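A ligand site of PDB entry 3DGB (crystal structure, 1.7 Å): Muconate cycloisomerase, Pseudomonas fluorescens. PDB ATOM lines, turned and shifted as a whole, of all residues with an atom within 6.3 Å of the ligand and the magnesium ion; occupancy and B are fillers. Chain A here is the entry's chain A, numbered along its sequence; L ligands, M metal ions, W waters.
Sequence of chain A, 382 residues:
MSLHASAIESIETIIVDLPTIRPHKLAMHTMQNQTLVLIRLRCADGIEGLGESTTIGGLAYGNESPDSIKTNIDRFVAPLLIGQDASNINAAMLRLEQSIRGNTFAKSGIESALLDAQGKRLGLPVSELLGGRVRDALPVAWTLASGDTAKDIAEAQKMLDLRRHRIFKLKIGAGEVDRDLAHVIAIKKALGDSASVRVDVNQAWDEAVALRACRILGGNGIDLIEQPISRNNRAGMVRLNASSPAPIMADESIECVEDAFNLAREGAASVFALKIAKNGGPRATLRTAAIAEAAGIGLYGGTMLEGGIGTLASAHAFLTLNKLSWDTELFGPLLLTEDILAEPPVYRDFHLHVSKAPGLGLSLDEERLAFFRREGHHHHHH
The side-chain amino group of Lys 171 is in salt-bridge range of an oxygen (O2) of the ligand.
O1 of the ligand lies close to OH of Tyr 61 (2.6 Å).
NZ of Lys 169 is in salt-bridge range of O2 of the ligand (2.8 Å).
An oxygen (O3) of the ligand sits at hydrogen-bond distance from a ring nitrogen (NE2) of His 24 (3.0 Å).
An oxygen (O1) of the ligand sits close to the side-chain amide nitrogen (ND2) of Asn 202.
The side-chain hydroxyl (OG1) of Thr 143 lies within hydrogen-bond range of an oxygen (O3) of the ligand (3.2 Å).
An oxygen (O1) of the ligand lies close to the side-chain amino group of Lys 275.
OH of Tyr 61 lies close to OD2 of Asp 251 (3.0 Å).
The backbone NH (N) of Asp 251 lies within hydrogen-bond range of the side-chain amide oxygen (OE1) of Gln 227 (2.8 Å).
NZ of Lys 171 sits close to OD2 of Asp 200 (2.9 Å).
NZ of Lys 171 lies within hydrogen-bond range of OD1 of Asn 202 (3.0 Å).
OH of Tyr 61 lies within hydrogen-bond range of NZ of Lys 275.
N of Met 31 sits at hydrogen-bond distance from O of His 24.
The side-chain hydroxyl (OH) of Tyr 300 lies within hydrogen-bond range of the side-chain carboxylate (OE1) of Glu 329 (2.7 Å).
The backbone carbonyl oxygen of Thr 303 sits close to the side-chain amino group of Lys 275 (3.3 Å).
Ile 56 touches the ligand.
O of Thr 303 touches C2 of the ligand, 3.3 Å away.
Leu 305 touches the ligand (CD2 to C4, 3.9 Å).
Glu 329 touches the ligand (OE2 to C2, 3.2 Å).
Phe 331 touches the ligand (CZ to O3, 3.6 Å).
Of the 24 residues printed, 14 come within 4 Å of the ligand.
The nearest printed residue that does not touch the ligand is Glu 226 (4.1 Å).
Merely in contact with the magnesium ion: Asn 202, Glu 252, Tyr 61 and Lys 169.
Within 4 Å of the magnesium ion: Tyr 61, Lys 169, Asp 200, Asn 202, Glu 226, Asp 251 and Glu 252.
The magnesium ion is bound by water W1 (1.8 Å), OD2 of Asp 251 (2.2 Å), OE2 of Glu 226 (2.3 Å), OD2 of Asp 200 (2.3 Å) and O1 of the ligand (2.4 Å).
Water W1 lies within hydrogen-bond range of the side-chain carboxylate (OE1) of Glu 252, the side-chain carboxylate (OD1) of Asp 200 and the side-chain amide nitrogen (ND2) of Asn 202.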
ATOM      1  N   HIS A  24     -17.132 -11.826   6.839  1.00  0.00           N
ATOM      2  CA  HIS A  24     -17.603 -12.011   8.209  1.00  0.00           C
ATOM      3  C   HIS A  24     -17.571 -13.516   8.474  1.00  0.00           C
ATOM      4  O   HIS A  24     -18.423 -14.262   7.990  1.00  0.00           O
ATOM      5  CB  HIS A  24     -19.029 -11.483   8.340  1.00  0.00           C
ATOM      6  CG  HIS A  24     -19.430 -11.141   9.739  1.00  0.00           C
ATOM      7  ND1 HIS A  24     -18.798 -10.166  10.488  1.00  0.00           N
ATOM      8  CD2 HIS A  24     -20.426 -11.617  10.522  1.00  0.00           C
ATOM      9  CE1 HIS A  24     -19.384 -10.055  11.666  1.00  0.00           C
ATOM     10  NE2 HIS A  24     -20.381 -10.931  11.710  1.00  0.00           N
ATOM     11  N   LEU A  26     -18.072 -16.771  10.603  1.00  0.00           N
ATOM     12  CA  LEU A  26     -18.782 -17.409  11.712  1.00  0.00           C
ATOM     13  C   LEU A  26     -18.250 -18.836  11.780  1.00  0.00           C
ATOM     14  O   LEU A  26     -17.579 -19.306  10.859  1.00  0.00           O
ATOM     15  CB  LEU A  26     -20.292 -17.430  11.468  1.00  0.00           C
ATOM     16  CG  LEU A  26     -21.015 -16.106  11.165  1.00  0.00           C
ATOM     17  CD1 LEU A  26     -22.493 -16.282  11.501  1.00  0.00           C
ATOM     18  CD2 LEU A  26     -20.433 -14.973  11.986  1.00  0.00           C
ATOM     19  N   MET A  28     -19.655 -21.661  11.370  1.00  0.00           N
ATOM     20  CA  MET A  28     -20.145 -22.546  10.302  1.00  0.00           C
ATOM     21  C   MET A  28     -20.133 -21.956   8.899  1.00  0.00           C
ATOM     22  O   MET A  28     -20.277 -22.690   7.920  1.00  0.00           O
ATOM     23  CB  MET A  28     -21.579 -22.986  10.624  1.00  0.00           C
ATOM     24  CG  MET A  28     -22.686 -22.035  10.119  1.00  0.00           C
ATOM     25  SD  MET A  28     -22.635 -20.338  10.767  1.00  0.00           S
ATOM     26  CE  MET A  28     -23.277 -20.618  12.427  1.00  0.00           C
ATOM     27  N   MET A  31     -19.293 -15.141   5.559  1.00  0.00           N
ATOM     28  CA  MET A  31     -20.076 -14.239   4.739  1.00  0.00           C
ATOM     29  C   MET A  31     -19.191 -13.393   3.823  1.00  0.00           C
ATOM     30  O   MET A  31     -18.195 -12.820   4.281  1.00  0.00           O
ATOM     31  CB  MET A  31     -20.904 -13.298   5.627  1.00  0.00           C
ATOM     32  CG  MET A  31     -21.975 -13.985   6.450  1.00  0.00           C
ATOM     33  SD  MET A  31     -22.795 -12.818   7.566  1.00  0.00           S
ATOM     34  CE  MET A  31     -23.767 -11.877   6.389  1.00  0.00           C
ATOM     35  N   ILE A  56     -28.642 -15.678   7.377  1.00  0.00           N
ATOM     36  CA  ILE A  56     -27.208 -15.719   7.152  1.00  0.00           C
ATOM     37  C   ILE A  56     -26.764 -16.987   6.416  1.00  0.00           C
ATOM     38  O   ILE A  56     -27.140 -18.092   6.790  1.00  0.00           O
ATOM     39  CB  ILE A  56     -26.433 -15.638   8.498  1.00  0.00           C
ATOM     40  CG1 ILE A  56     -26.681 -14.284   9.161  1.00  0.00           C
ATOM     41  CG2 ILE A  56     -24.946 -15.873   8.263  1.00  0.00           C
ATOM     42  CD1 ILE A  56     -26.097 -14.162  10.558  1.00  0.00           C
ATOM     43  N   TYR A  61     -27.243 -21.268   8.337  1.00  0.00           N
ATOM     44  CA  TYR A  61     -27.623 -20.848   9.684  1.00  0.00           C
ATOM     45  C   TYR A  61     -28.968 -21.435  10.110  1.00  0.00           C
ATOM     46  O   TYR A  61     -29.062 -22.108  11.141  1.00  0.00           O
ATOM     47  CB  TYR A  61     -27.676 -19.322   9.767  1.00  0.00           C
ATOM     48  CG  TYR A  61     -27.732 -18.798  11.182  1.00  0.00           C
ATOM     49  CD1 TYR A  61     -26.587 -18.345  11.829  1.00  0.00           C
ATOM     50  CD2 TYR A  61     -28.937 -18.781  11.884  1.00  0.00           C
ATOM     51  CE1 TYR A  61     -26.635 -17.890  13.142  1.00  0.00           C
ATOM     52  CE2 TYR A  61     -28.994 -18.331  13.196  1.00  0.00           C
ATOM     53  CZ  TYR A  61     -27.845 -17.882  13.812  1.00  0.00           C
ATOM     54  OH  TYR A  61     -27.912 -17.433  15.111  1.00  0.00           O
ATOM     55  N   THR A 143     -19.314  -6.882  16.125  1.00  0.00           N
ATOM     56  CA  THR A 143     -18.713  -8.205  16.039  1.00  0.00           C
ATOM     57  C   THR A 143     -17.379  -8.188  15.314  1.00  0.00           C
ATOM     58  O   THR A 143     -17.242  -7.596  14.241  1.00  0.00           O
ATOM     59  CB  THR A 143     -19.650  -9.201  15.326  1.00  0.00           C
ATOM     60  OG1 THR A 143     -20.827  -9.383  16.115  1.00  0.00           O
ATOM     61  CG2 THR A 143     -18.957 -10.537  15.125  1.00  0.00           C
ATOM     62  N   LYS A 169     -18.190  -8.410  20.252  1.00  0.00           N
ATOM     63  CA  LYS A 169     -18.595  -9.809  20.195  1.00  0.00           C
ATOM     64  C   LYS A 169     -17.625 -10.540  19.275  1.00  0.00           C
ATOM     65  O   LYS A 169     -17.449 -10.151  18.124  1.00  0.00           O
ATOM     66  CB  LYS A 169     -20.020  -9.898  19.664  1.00  0.00           C
ATOM     67  CG  LYS A 169     -20.476 -11.284  19.246  1.00  0.00           C
ATOM     68  CD  LYS A 169     -21.967 -11.268  18.944  1.00  0.00           C
ATOM     69  CE  LYS A 169     -22.407 -12.517  18.217  1.00  0.00           C
ATOM     70  NZ  LYS A 169     -23.886 -12.622  18.167  1.00  0.00           N
ATOM     71  N   LYS A 171     -16.522 -13.932  17.267  1.00  0.00           N
ATOM     72  CA  LYS A 171     -16.969 -15.184  16.688  1.00  0.00           C
ATOM     73  C   LYS A 171     -15.861 -16.223  16.789  1.00  0.00           C
ATOM     74  O   LYS A 171     -14.760 -16.014  16.296  1.00  0.00           O
ATOM     75  CB  LYS A 171     -17.303 -14.989  15.206  1.00  0.00           C
ATOM     76  CG  LYS A 171     -18.531 -14.161  14.950  1.00  0.00           C
ATOM     77  CD  LYS A 171     -19.736 -14.864  15.514  1.00  0.00           C
ATOM     78  CE  LYS A 171     -21.007 -14.160  15.143  1.00  0.00           C
ATOM     79  NZ  LYS A 171     -22.151 -15.029  15.506  1.00  0.00           N
ATOM     80  N   ASP A 200     -19.225 -15.697  20.875  1.00  0.00           N
ATOM     81  CA  ASP A 200     -20.369 -16.435  20.336  1.00  0.00           C
ATOM     82  C   ASP A 200     -19.736 -17.637  19.648  1.00  0.00           C
ATOM     83  O   ASP A 200     -18.935 -17.473  18.724  1.00  0.00           O
ATOM     84  CB  ASP A 200     -21.129 -15.599  19.302  1.00  0.00           C
ATOM     85  CG  ASP A 200     -22.401 -16.289  18.818  1.00  0.00           C
ATOM     86  OD1 ASP A 200     -22.593 -17.485  19.128  1.00  0.00           O
ATOM     87  OD2 ASP A 200     -23.210 -15.641  18.118  1.00  0.00           O
ATOM     88  N   ASN A 202     -21.622 -20.108  18.311  1.00  0.00           N
ATOM     89  CA  ASN A 202     -22.583 -20.624  17.349  1.00  0.00           C
ATOM     90  C   ASN A 202     -22.765 -22.144  17.400  1.00  0.00           C
ATOM     91  O   ASN A 202     -22.731 -22.826  16.368  1.00  0.00           O
ATOM     92  CB  ASN A 202     -22.196 -20.198  15.924  1.00  0.00           C
ATOM     93  CG  ASN A 202     -22.433 -18.710  15.664  1.00  0.00           C
ATOM     94  OD1 ASN A 202     -21.492 -17.931  15.500  1.00  0.00           O
ATOM     95  ND2 ASN A 202     -23.707 -18.311  15.648  1.00  0.00           N
ATOM     96  N   GLU A 226     -22.022 -16.771  24.390  1.00  0.00           N
ATOM     97  CA  GLU A 226     -23.221 -17.056  23.605  1.00  0.00           C
ATOM     98  C   GLU A 226     -23.222 -18.428  22.936  1.00  0.00           C
ATOM     99  O   GLU A 226     -22.258 -18.795  22.257  1.00  0.00           O
ATOM    100  CB  GLU A 226     -23.402 -15.966  22.542  1.00  0.00           C
ATOM    101  CG  GLU A 226     -24.697 -16.038  21.769  1.00  0.00           C
ATOM    102  CD  GLU A 226     -24.825 -14.921  20.732  1.00  0.00           C
ATOM    103  OE1 GLU A 226     -24.017 -13.971  20.793  1.00  0.00           O
ATOM    104  OE2 GLU A 226     -25.721 -14.997  19.871  1.00  0.00           O
ATOM    105  N   GLN A 227     -24.311 -19.165  23.162  1.00  0.00           N
ATOM    106  CA  GLN A 227     -24.562 -20.498  22.608  1.00  0.00           C
ATOM    107  C   GLN A 227     -23.300 -21.336  22.379  1.00  0.00           C
ATOM    108  O   GLN A 227     -22.936 -21.637  21.246  1.00  0.00           O
ATOM    109  CB  GLN A 227     -25.347 -20.363  21.297  1.00  0.00           C
ATOM    110  CG  GLN A 227     -26.080 -21.615  20.816  1.00  0.00           C
ATOM    111  CD  GLN A 227     -27.338 -21.926  21.618  1.00  0.00           C
ATOM    112  OE1 GLN A 227     -28.128 -21.035  21.926  1.00  0.00           O
ATOM    113  NE2 GLN A 227     -27.532 -23.208  21.932  1.00  0.00           N
ATOM    114  N   ASP A 251     -29.189 -18.441  22.047  1.00  0.00           N
ATOM    115  CA  ASP A 251     -29.535 -17.780  20.792  1.00  0.00           C
ATOM    116  C   ASP A 251     -30.222 -18.807  19.915  1.00  0.00           C
ATOM    117  O   ASP A 251     -31.450 -18.827  19.831  1.00  0.00           O
ATOM    118  CB  ASP A 251     -28.288 -17.211  20.096  1.00  0.00           C
ATOM    119  CG  ASP A 251     -28.612 -16.602  18.735  1.00  0.00           C
ATOM    120  OD1 ASP A 251     -29.808 -16.312  18.496  1.00  0.00           O
ATOM    121  OD2 ASP A 251     -27.693 -16.395  17.917  1.00  0.00           O
ATOM    122  N   GLU A 252     -29.449 -19.668  19.270  1.00  0.00           N
ATOM    123  CA  GLU A 252     -30.026 -20.694  18.413  1.00  0.00           C
ATOM    124  C   GLU A 252     -30.996 -21.598  19.171  1.00  0.00           C
ATOM    125  O   GLU A 252     -31.891 -22.200  18.562  1.00  0.00           O
ATOM    126  CB  GLU A 252     -28.907 -21.532  17.766  1.00  0.00           C
ATOM    127  CG  GLU A 252     -28.133 -20.781  16.692  1.00  0.00           C
ATOM    128  CD  GLU A 252     -26.839 -20.158  17.190  1.00  0.00           C
ATOM    129  OE1 GLU A 252     -26.809 -19.685  18.347  1.00  0.00           O
ATOM    130  OE2 GLU A 252     -25.860 -20.120  16.421  1.00  0.00           O
ATOM    131  N   LYS A 275     -34.447 -12.067  18.932  1.00  0.00           N
ATOM    132  CA  LYS A 275     -34.376 -11.859  17.493  1.00  0.00           C
ATOM    133  C   LYS A 275     -35.758 -11.955  16.875  1.00  0.00           C
ATOM    134  O   LYS A 275     -36.449 -12.964  17.024  1.00  0.00           O
ATOM    135  CB  LYS A 275     -33.432 -12.884  16.859  1.00  0.00           C
ATOM    136  CG  LYS A 275     -32.003 -12.755  17.349  1.00  0.00           C
ATOM    137  CD  LYS A 275     -31.057 -13.731  16.647  1.00  0.00           C
ATOM    138  CE  LYS A 275     -29.627 -13.512  17.120  1.00  0.00           C
ATOM    139  NZ  LYS A 275     -28.658 -14.377  16.397  1.00  0.00           N
ATOM    140  N   TYR A 300     -30.999  -9.379  25.646  1.00  0.00           N
ATOM    141  CA  TYR A 300     -30.014  -8.925  24.665  1.00  0.00           C
ATOM    142  C   TYR A 300     -30.759  -8.690  23.365  1.00  0.00           C
ATOM    143  O   TYR A 300     -31.518  -9.559  22.917  1.00  0.00           O
ATOM    144  CB  TYR A 300     -28.962 -10.017  24.468  1.00  0.00           C
ATOM    145  CG  TYR A 300     -27.890  -9.710  23.444  1.00  0.00           C
ATOM    146  CD1 TYR A 300     -26.926  -8.736  23.698  1.00  0.00           C
ATOM    147  CD2 TYR A 300     -27.782 -10.480  22.292  1.00  0.00           C
ATOM    148  CE1 TYR A 300     -25.861  -8.543  22.826  1.00  0.00           C
ATOM    149  CE2 TYR A 300     -26.715 -10.291  21.411  1.00  0.00           C
ATOM    150  CZ  TYR A 300     -25.755  -9.333  21.683  1.00  0.00           C
ATOM    151  OH  TYR A 300     -24.670  -9.189  20.862  1.00  0.00           O
ATOM    152  N   GLY A 302     -30.893  -8.988  19.858  1.00  0.00           N
ATOM    153  CA  GLY A 302     -30.171  -9.677  18.802  1.00  0.00           C
ATOM    154  C   GLY A 302     -30.499  -9.298  17.374  1.00  0.00           C
ATOM    155  O   GLY A 302     -31.465  -8.569  17.102  1.00  0.00           O
ATOM    156  N   THR A 303     -29.701  -9.820  16.456  1.00  0.00           N
ATOM    157  CA  THR A 303     -29.897  -9.550  15.036  1.00  0.00           C
ATOM    158  C   THR A 303     -29.504 -10.747  14.185  1.00  0.00           C
ATOM    159  O   THR A 303     -28.726 -11.615  14.625  1.00  0.00           O
ATOM    160  CB  THR A 303     -29.036  -8.330  14.580  1.00  0.00           C
ATOM    161  OG1 THR A 303     -29.367  -7.980  13.232  1.00  0.00           O
ATOM    162  CG2 THR A 303     -27.552  -8.663  14.649  1.00  0.00           C
ATOM    163  N   MET A 304     -30.057 -10.818  12.978  1.00  0.00           N
ATOM    164  CA  MET A 304     -29.699 -11.866  12.026  1.00  0.00           C
ATOM    165  C   MET A 304     -28.989 -11.134  10.884  1.00  0.00           C
ATOM    166  O   MET A 304     -28.954 -11.605   9.745  1.00  0.00           O
ATOM    167  CB  MET A 304     -30.932 -12.608  11.509  1.00  0.00           C
ATOM    168  CG  MET A 304     -31.480 -13.685  12.468  1.00  0.00           C
ATOM    169  SD  MET A 304     -30.296 -14.968  12.965  1.00  0.00           S
ATOM    170  CE  MET A 304     -29.669 -15.509  11.324  1.00  0.00           C
ATOM    171  N   LEU A 305     -28.427  -9.972  11.220  1.00  0.00           N
ATOM    172  CA  LEU A 305     -27.704  -9.113  10.286  1.00  0.00           C
ATOM    173  C   LEU A 305     -28.606  -8.483   9.225  1.00  0.00           C
ATOM    174  O   LEU A 305     -28.268  -8.413   8.041  1.00  0.00           O
ATOM    175  CB  LEU A 305     -26.543  -9.875   9.628  1.00  0.00           C
ATOM    176  CG  LEU A 305     -25.461 -10.322  10.623  1.00  0.00           C
ATOM    177  CD1 LEU A 305     -24.327 -11.021   9.883  1.00  0.00           C
ATOM    178  CD2 LEU A 305     -24.926  -9.110  11.383  1.00  0.00           C
ATOM    179  N   GLU A 329     -26.985  -5.818  19.538  1.00  0.00           N
ATOM    180  CA  GLU A 329     -26.028  -6.011  18.458  1.00  0.00           C
ATOM    181  C   GLU A 329     -26.681  -5.560  17.154  1.00  0.00           C
ATOM    182  O   GLU A 329     -26.505  -6.187  16.104  1.00  0.00           O
ATOM    183  CB  GLU A 329     -25.610  -7.481  18.353  1.00  0.00           C
ATOM    184  CG  GLU A 329     -26.776  -8.463  18.352  1.00  0.00           C
ATOM    185  CD  GLU A 329     -26.343  -9.900  18.100  1.00  0.00           C
ATOM    186  OE1 GLU A 329     -25.193 -10.249  18.467  1.00  0.00           O
ATOM    187  OE2 GLU A 329     -27.149 -10.686  17.555  1.00  0.00           O
ATOM    188  N   PHE A 331     -26.183  -3.831  14.586  1.00  0.00           N
ATOM    189  CA  PHE A 331     -25.208  -3.193  13.712  1.00  0.00           C
ATOM    190  C   PHE A 331     -25.280  -3.657  12.266  1.00  0.00           C
ATOM    191  O   PHE A 331     -24.431  -3.310  11.443  1.00  0.00           O
ATOM    192  CB  PHE A 331     -23.795  -3.440  14.256  1.00  0.00           C
ATOM    193  CG  PHE A 331     -23.361  -4.880  14.210  1.00  0.00           C
ATOM    194  CD1 PHE A 331     -22.893  -5.451  13.026  1.00  0.00           C
ATOM    195  CD2 PHE A 331     -23.442  -5.683  15.349  1.00  0.00           C
ATOM    196  CE1 PHE A 331     -22.509  -6.791  12.976  1.00  0.00           C
ATOM    197  CE2 PHE A 331     -23.061  -7.019  15.309  1.00  0.00           C
ATOM    198  CZ  PHE A 331     -22.587  -7.577  14.121  1.00  0.00           C
ATOM    199  N   LEU A 335     -22.618  -3.238   8.637  1.00  0.00           N
ATOM    200  CA  LEU A 335     -21.818  -4.290   8.008  1.00  0.00           C
ATOM    201  C   LEU A 335     -22.030  -4.246   6.494  1.00  0.00           C
ATOM    202  O   LEU A 335     -21.173  -4.679   5.723  1.00  0.00           O
ATOM    203  CB  LEU A 335     -22.218  -5.661   8.565  1.00  0.00           C
ATOM    204  CG  LEU A 335     -21.429  -6.888   8.092  1.00  0.00           C
ATOM    205  CD1 LEU A 335     -19.961  -6.754   8.454  1.00  0.00           C
ATOM    206  CD2 LEU A 335     -22.029  -8.137   8.739  1.00  0.00           C
HETATM  207  C1  LIG L   1     -25.378 -14.809  15.371  1.00  0.00           C
HETATM  208  O1  LIG L   1     -25.798 -15.962  15.572  1.00  0.00           O
HETATM  209  O2  LIG L   1     -24.479 -14.244  16.020  1.00  0.00           O
HETATM  210  C2  LIG L   1     -25.436 -11.618  15.077  1.00  0.00           C
HETATM  211  C3  LIG L   1     -24.358 -10.861  14.872  1.00  0.00           C
HETATM  212  C4  LIG L   1     -23.502 -11.539  14.111  1.00  0.00           C
HETATM  213  O3  LIG L   1     -22.328 -11.204  13.944  1.00  0.00           O
HETATM  214  O4  LIG L   1     -24.044 -12.669  13.538  1.00  0.00           O
HETATM  215  C5  LIG L   1     -25.434 -12.600  13.901  1.00  0.00           C
HETATM  216  C6  LIG L   1     -26.029 -14.018  14.195  1.00  0.00           C
HETATM  217 MG    MG M   1     -25.447 -16.274  17.942  1.00  0.00          MG
HETATM  218  O   HOH W   1     -25.071 -17.889  18.619  1.00  0.00           O
